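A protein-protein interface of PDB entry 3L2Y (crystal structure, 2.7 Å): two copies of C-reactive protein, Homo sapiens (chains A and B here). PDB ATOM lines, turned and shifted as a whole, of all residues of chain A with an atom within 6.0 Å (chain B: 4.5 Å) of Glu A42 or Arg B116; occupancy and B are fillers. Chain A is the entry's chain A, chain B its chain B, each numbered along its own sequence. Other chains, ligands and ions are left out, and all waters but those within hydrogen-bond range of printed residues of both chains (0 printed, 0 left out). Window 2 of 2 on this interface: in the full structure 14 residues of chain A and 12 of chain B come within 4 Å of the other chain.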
ATOM      1  N   TYR A  40      16.739  -5.084  13.898  1.00  0.00           N
ATOM      2  CA  TYR A  40      16.729  -5.317  15.325  1.00  0.00           C
ATOM      3  C   TYR A  40      17.955  -4.660  15.940  1.00  0.00           C
ATOM      4  O   TYR A  40      19.078  -5.058  15.648  1.00  0.00           O
ATOM      5  CB  TYR A  40      16.759  -6.820  15.586  1.00  0.00           C
ATOM      6  CG  TYR A  40      16.572  -7.208  17.029  1.00  0.00           C
ATOM      7  CD1 TYR A  40      16.072  -6.311  17.948  1.00  0.00           C
ATOM      8  CD2 TYR A  40      16.895  -8.480  17.472  1.00  0.00           C
ATOM      9  CE1 TYR A  40      15.889  -6.669  19.263  1.00  0.00           C
ATOM     10  CE2 TYR A  40      16.710  -8.844  18.791  1.00  0.00           C
ATOM     11  CZ  TYR A  40      16.205  -7.933  19.677  1.00  0.00           C
ATOM     12  OH  TYR A  40      16.022  -8.276  20.983  1.00  0.00           O
ATOM     13  N   THR A  41      17.744  -3.652  16.784  1.00  0.00           N
ATOM     14  CA  THR A  41      18.866  -2.968  17.399  1.00  0.00           C
ATOM     15  C   THR A  41      18.483  -2.501  18.791  1.00  0.00           C
ATOM     16  O   THR A  41      17.304  -2.401  19.090  1.00  0.00           O
ATOM     17  CB  THR A  41      19.322  -1.776  16.557  1.00  0.00           C
ATOM     18  OG1 THR A  41      20.375  -1.086  17.231  1.00  0.00           O
ATOM     19  CG2 THR A  41      18.183  -0.832  16.352  1.00  0.00           C
ATOM     20  N   GLU A  42      19.474  -2.247  19.646  1.00  0.00           N
ATOM     21  CA  GLU A  42      19.203  -1.691  20.975  1.00  0.00           C
ATOM     22  C   GLU A  42      19.595  -0.215  21.062  1.00  0.00           C
ATOM     23  O   GLU A  42      19.601   0.377  22.139  1.00  0.00           O
ATOM     24  CB  GLU A  42      19.878  -2.509  22.088  1.00  0.00           C
ATOM     25  CG  GLU A  42      19.238  -3.880  22.285  1.00  0.00           C
ATOM     26  CD  GLU A  42      19.796  -4.672  23.454  1.00  0.00           C
ATOM     27  OE1 GLU A  42      20.707  -4.160  24.163  1.00  0.00           O
ATOM     28  OE2 GLU A  42      19.304  -5.817  23.639  1.00  0.00           O
ATOM     29  N   LEU A  43      19.909   0.379  19.919  1.00  0.00           N
ATOM     30  CA  LEU A  43      20.406   1.741  19.884  1.00  0.00           C
ATOM     31  C   LEU A  43      19.345   2.802  20.201  1.00  0.00           C
ATOM     32  O   LEU A  43      19.686   3.912  20.581  1.00  0.00           O
ATOM     33  CB  LEU A  43      21.036   2.023  18.524  1.00  0.00           C
ATOM     34  CG  LEU A  43      22.534   1.803  18.382  1.00  0.00           C
ATOM     35  CD1 LEU A  43      22.989   0.608  19.194  1.00  0.00           C
ATOM     36  CD2 LEU A  43      22.845   1.623  16.909  1.00  0.00           C
ATOM     37  N   SER A  44      18.072   2.459  20.055  1.00  0.00           N
ATOM     38  CA  SER A  44      16.983   3.431  20.143  1.00  0.00           C
ATOM     39  C   SER A  44      17.021   4.265  21.418  1.00  0.00           C
ATOM     40  O   SER A  44      16.651   5.446  21.421  1.00  0.00           O
ATOM     41  CB  SER A  44      15.635   2.722  20.040  1.00  0.00           C
ATOM     42  OG  SER A  44      15.634   1.767  18.981  1.00  0.00           O
ATOM     43  N   SER A  45      17.485   3.646  22.497  1.00  0.00           N
ATOM     44  CA  SER A  45      17.561   4.303  23.795  1.00  0.00           C
ATOM     45  C   SER A  45      18.693   5.324  23.882  1.00  0.00           C
ATOM     46  O   SER A  45      18.587   6.307  24.619  1.00  0.00           O
ATOM     47  CB  SER A  45      17.742   3.255  24.893  1.00  0.00           C
ATOM     48  OG  SER A  45      18.942   2.519  24.704  1.00  0.00           O
ATOM     49  N   THR A  46      19.771   5.091  23.133  1.00  0.00           N
ATOM     50  CA  THR A  46      20.995   5.872  23.304  1.00  0.00           C
ATOM     51  C   THR A  46      21.355   6.868  22.179  1.00  0.00           C
ATOM     52  O   THR A  46      21.968   7.897  22.444  1.00  0.00           O
ATOM     53  CB  THR A  46      22.198   4.961  23.617  1.00  0.00           C
ATOM     54  OG1 THR A  46      22.605   4.278  22.431  1.00  0.00           O
ATOM     55  CG2 THR A  46      21.815   3.934  24.667  1.00  0.00           C
ATOM     56  N   VAL A  91      11.925  -3.393  23.109  1.00  0.00           N
ATOM     57  CA  VAL A  91      13.097  -4.131  22.665  1.00  0.00           C
ATOM     58  C   VAL A  91      12.693  -5.437  21.977  1.00  0.00           C
ATOM     59  O   VAL A  91      12.533  -6.481  22.606  1.00  0.00           O
ATOM     60  CB  VAL A  91      14.094  -4.407  23.836  1.00  0.00           C
ATOM     61  CG1 VAL A  91      13.358  -4.908  25.073  1.00  0.00           C
ATOM     62  CG2 VAL A  91      15.205  -5.386  23.408  1.00  0.00           C
ATOM     63  N   VAL A 153      23.742  -0.811  14.578  1.00  0.00           N
ATOM     64  CA  VAL A 153      24.393  -1.898  15.290  1.00  0.00           C
ATOM     65  C   VAL A 153      23.330  -2.914  15.646  1.00  0.00           C
ATOM     66  O   VAL A 153      22.452  -2.658  16.468  1.00  0.00           O
ATOM     67  CB  VAL A 153      25.145  -1.434  16.558  1.00  0.00           C
ATOM     68  CG1 VAL A 153      25.891  -2.609  17.182  1.00  0.00           C
ATOM     69  CG2 VAL A 153      26.113  -0.337  16.224  1.00  0.00           C
ATOM     70  N   LEU A 204      17.011 -13.631  13.473  1.00  0.00           N
ATOM     71  CA  LEU A 204      16.511 -13.749  14.852  1.00  0.00           C
ATOM     72  C   LEU A 204      14.994 -13.639  14.958  1.00  0.00           C
ATOM     73  O   LEU A 204      14.407 -13.992  15.980  1.00  0.00           O
ATOM     74  CB  LEU A 204      17.133 -12.684  15.747  1.00  0.00           C
ATOM     75  CG  LEU A 204      18.647 -12.829  15.814  1.00  0.00           C
ATOM     76  CD1 LEU A 204      19.320 -11.669  16.500  1.00  0.00           C
ATOM     77  CD2 LEU A 204      18.959 -14.109  16.523  1.00  0.00           C
ATOM     78  N   PHE B  84      23.837  -6.757  28.942  1.00  0.00           N
ATOM     79  CA  PHE B  84      22.506  -6.840  28.361  1.00  0.00           C
ATOM     80  C   PHE B  84      21.535  -6.270  29.368  1.00  0.00           C
ATOM     81  O   PHE B  84      21.112  -6.978  30.264  1.00  0.00           O
ATOM     82  CB  PHE B  84      22.142  -8.290  28.017  1.00  0.00           C
ATOM     83  CG  PHE B  84      22.903  -8.831  26.845  1.00  0.00           C
ATOM     84  CD1 PHE B  84      22.495  -8.558  25.557  1.00  0.00           C
ATOM     85  CD2 PHE B  84      24.059  -9.565  27.029  1.00  0.00           C
ATOM     86  CE1 PHE B  84      23.208  -9.018  24.483  1.00  0.00           C
ATOM     87  CE2 PHE B  84      24.783 -10.029  25.947  1.00  0.00           C
ATOM     88  CZ  PHE B  84      24.350  -9.751  24.676  1.00  0.00           C
ATOM     89  N   GLU B  85      21.218  -4.979  29.235  1.00  0.00           N
ATOM     90  CA  GLU B  85      20.355  -4.269  30.185  1.00  0.00           C
ATOM     91  C   GLU B  85      19.014  -4.941  30.387  1.00  0.00           C
ATOM     92  O   GLU B  85      18.426  -5.466  29.451  1.00  0.00           O
ATOM     93  CB  GLU B  85      20.050  -2.856  29.699  1.00  0.00           C
ATOM     94  CG  GLU B  85      21.016  -1.809  30.140  1.00  0.00           C
ATOM     95  CD  GLU B  85      22.241  -1.787  29.269  1.00  0.00           C
ATOM     96  OE1 GLU B  85      22.298  -2.583  28.288  1.00  0.00           O
ATOM     97  OE2 GLU B  85      23.138  -0.966  29.572  1.00  0.00           O
ATOM     98  N   VAL B  86      18.519  -4.886  31.614  1.00  0.00           N
ATOM     99  CA  VAL B  86      17.193  -5.383  31.922  1.00  0.00           C
ATOM    100  C   VAL B  86      16.517  -4.457  32.917  1.00  0.00           C
ATOM    101  O   VAL B  86      16.842  -4.446  34.107  1.00  0.00           O
ATOM    102  CB  VAL B  86      17.229  -6.808  32.488  1.00  0.00           C
ATOM    103  CG1 VAL B  86      15.902  -7.159  33.118  1.00  0.00           C
ATOM    104  CG2 VAL B  86      17.560  -7.780  31.397  1.00  0.00           C
ATOM    105  N   PHE B 109      22.305 -13.444  23.255  1.00  0.00           N
ATOM    106  CA  PHE B 109      21.792 -13.668  24.593  1.00  0.00           C
ATOM    107  C   PHE B 109      20.287 -13.846  24.501  1.00  0.00           C
ATOM    108  O   PHE B 109      19.575 -12.957  24.047  1.00  0.00           O
ATOM    109  CB  PHE B 109      22.173 -12.505  25.502  1.00  0.00           C
ATOM    110  CG  PHE B 109      22.235 -12.856  26.966  1.00  0.00           C
ATOM    111  CD1 PHE B 109      23.425 -13.244  27.543  1.00  0.00           C
ATOM    112  CD2 PHE B 109      21.112 -12.778  27.767  1.00  0.00           C
ATOM    113  CE1 PHE B 109      23.493 -13.547  28.881  1.00  0.00           C
ATOM    114  CE2 PHE B 109      21.179 -13.086  29.107  1.00  0.00           C
ATOM    115  CZ  PHE B 109      22.370 -13.469  29.664  1.00  0.00           C
ATOM    116  N   LYS B 114      13.440 -15.583  24.057  1.00  0.00           N
ATOM    117  CA  LYS B 114      13.425 -14.397  23.200  1.00  0.00           C
ATOM    118  C   LYS B 114      14.832 -13.842  23.037  1.00  0.00           C
ATOM    119  O   LYS B 114      15.516 -13.596  24.017  1.00  0.00           O
ATOM    120  CB  LYS B 114      12.513 -13.313  23.784  1.00  0.00           C
ATOM    121  CG  LYS B 114      11.087 -13.761  24.095  1.00  0.00           C
ATOM    122  CD  LYS B 114      10.241 -13.965  22.839  1.00  0.00           C
ATOM    123  CE  LYS B 114       8.783 -14.265  23.196  1.00  0.00           C
ATOM    124  NZ  LYS B 114       7.924 -14.396  21.987  1.00  0.00           N
ATOM    125  N   PRO B 115      15.263 -13.618  21.798  1.00  0.00           N
ATOM    126  CA  PRO B 115      16.626 -13.151  21.564  1.00  0.00           C
ATOM    127  C   PRO B 115      16.807 -11.664  21.885  1.00  0.00           C
ATOM    128  O   PRO B 115      15.964 -10.838  21.550  1.00  0.00           O
ATOM    129  CB  PRO B 115      16.810 -13.372  20.061  1.00  0.00           C
ATOM    130  CG  PRO B 115      15.437 -13.534  19.501  1.00  0.00           C
ATOM    131  CD  PRO B 115      14.436 -13.484  20.596  1.00  0.00           C
ATOM    132  N   ARG B 116      17.906 -11.340  22.543  1.00  0.00           N
ATOM    133  CA  ARG B 116      18.334  -9.970  22.681  1.00  0.00           C
ATOM    134  C   ARG B 116      19.058  -9.673  21.388  1.00  0.00           C
ATOM    135  O   ARG B 116      19.344 -10.575  20.607  1.00  0.00           O
ATOM    136  CB  ARG B 116      19.300  -9.821  23.867  1.00  0.00           C
ATOM    137  CG  ARG B 116      18.658 -10.074  25.219  1.00  0.00           C
ATOM    138  CD  ARG B 116      17.587  -9.028  25.503  1.00  0.00           C
ATOM    139  NE  ARG B 116      18.224  -7.739  25.697  1.00  0.00           N
ATOM    140  CZ  ARG B 116      18.540  -7.243  26.886  1.00  0.00           C
ATOM    141  NH1 ARG B 116      18.231  -7.920  27.987  1.00  0.00           N
ATOM    142  NH2 ARG B 116      19.150  -6.064  26.975  1.00  0.00           N
ATOM    143  N   VAL B 117      19.369  -8.411  21.158  1.00  0.00           N
ATOM    144  CA  VAL B 117      20.121  -8.051  19.978  1.00  0.00           C
ATOM    145  C   VAL B 117      21.502  -8.718  19.976  1.00  0.00           C
ATOM    146  O   VAL B 117      22.008  -9.121  21.000  1.00  0.00           O
ATOM    147  CB  VAL B 117      20.259  -6.523  19.842  1.00  0.00           C
ATOM    148  CG1 VAL B 117      21.361  -6.015  20.729  1.00  0.00           C
ATOM    149  CG2 VAL B 117      20.567  -6.162  18.408  1.00  0.00           C
ATOM    150  N   ARG B 118      22.103  -8.865  18.807  1.00  0.00           N
ATOM    151  CA  ARG B 118      23.424  -9.438  18.734  1.00  0.00           C
ATOM    152  C   ARG B 118      24.498  -8.400  19.048  1.00  0.00           C
ATOM    153  O   ARG B 118      24.363  -7.214  18.720  1.00  0.00           O
ATOM    154  CB  ARG B 118      23.648 -10.033  17.361  1.00  0.00           C
ATOM    155  CG  ARG B 118      22.925 -11.344  17.146  1.00  0.00           C
ATOM    156  CD  ARG B 118      22.994 -11.812  15.687  1.00  0.00           C
ATOM    157  NE  ARG B 118      22.641 -13.226  15.541  1.00  0.00           N
ATOM    158  CZ  ARG B 118      21.809 -13.712  14.624  1.00  0.00           C
ATOM    159  NH1 ARG B 118      21.220 -12.903  13.752  1.00  0.00           N
ATOM    160  NH2 ARG B 118      21.566 -15.015  14.576  1.00  0.00           N
ATOM    161  N   LYS B 119      25.564  -8.842  19.702  1.00  0.00           N
ATOM    162  CA  LYS B 119      26.650  -7.937  20.059  1.00  0.00           C
ATOM    163  C   LYS B 119      28.012  -8.557  19.743  1.00  0.00           C
ATOM    164  O   LYS B 119      28.096  -9.701  19.309  1.00  0.00           O
ATOM    165  CB  LYS B 119      26.570  -7.538  21.540  1.00  0.00           C
ATOM    166  CG  LYS B 119      25.228  -6.934  21.943  1.00  0.00           C
ATOM    167  CD  LYS B 119      25.298  -6.212  23.291  1.00  0.00           C
ATOM    168  CE  LYS B 119      24.004  -5.459  23.583  1.00  0.00           C
ATOM    169  NZ  LYS B 119      24.118  -4.441  24.667  1.00  0.00           N
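O of Pro B115 sits at hydrogen-bond distance from OH of Tyr A40 (2.6 Å). The side-chain hydroxyl (OH) of Tyr A40 sits at hydrogen-bond distance from the backbone NH (N) of Val B117, at 3.4 Å. The side-chain carboxylate (OE2) of Glu A42 is in salt-bridge range of the guanidinium group (NE) of Arg B116, 3.0 Å away. The side-chain carboxylate of Glu A42 is in salt-bridge range of the side-chain amino group of Lys B119, 3.5 Å away.
No position is printed for both chains. Of the 9 pairs that touch across the chains among the printed residues, none has its exchanged pair printed and touching as well.
Of the printed residues of chain B, Thr A41 touches Val B117 (3.8 Å). Of chain B, only Arg B116 (3.0 Å), Val B117 (3.4 Å) and Lys B119 (3.5 Å) come within 4 Å of Glu A42. Of the printed residues of chain B, Leu A204 touches Pro B115 (3.7 Å) and Arg B118 (3.3 Å). Val B86 touches none of the printed residues of chain A. Of the printed residues of chain A, Pro B115 touches Tyr A40 and Leu A204. Of chain A, only Tyr A40 (3.3 Å) and Glu A42 (3.0 Å) come within 4 Å of Arg B116. Printed residues of chain A within 4 Å of Lys B119: Glu A42. The nearest printed residue of chain B that does not touch Tyr A40 is Arg B118 (5.4 Å).
OH of Tyr A40 touches CA of Arg B116, 3.3 Å away. Val B117 touches Thr A41. Glu A42 touches Val B117. Leu A204 touches Pro B115 (O to CG, 3.7 Å). Arg B118 touches Leu A204 (NH1 to CG, 3.3 Å).
The side-chain hydroxyl of Thr A41 sits at hydrogen-bond distance from the backbone NH of Leu A43, 3.1 Å away. OG1 of Thr A41 is in hydrogen-bond range of O of Val A153. The backbone carbonyl oxygen (O) of Glu A42 sits at hydrogen-bond distance from the side-chain hydroxyl (OG) of Ser A45, at 3.4 Å. The backbone carbonyl oxygen of Glu B85 is in hydrogen-bond range of the guanidinium group of Arg B116 (2.6 Å). The backbone NH of Arg B116 sits at hydrogen-bond distance from the backbone carbonyl oxygen of Phe B109, 2.8 Å away.
Of the 10 printed residues of chain B, 5 touch a printed residue of chain A. Hydrophobic or aromatic side chains of chain B within 4 Å of the printed part of chain A: Pro B115 and Val B117. Of the 10 printed residues of chain A, 4 touch a printed residue of chain B. Among the printed residues, 9 pairs touch across the chains.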
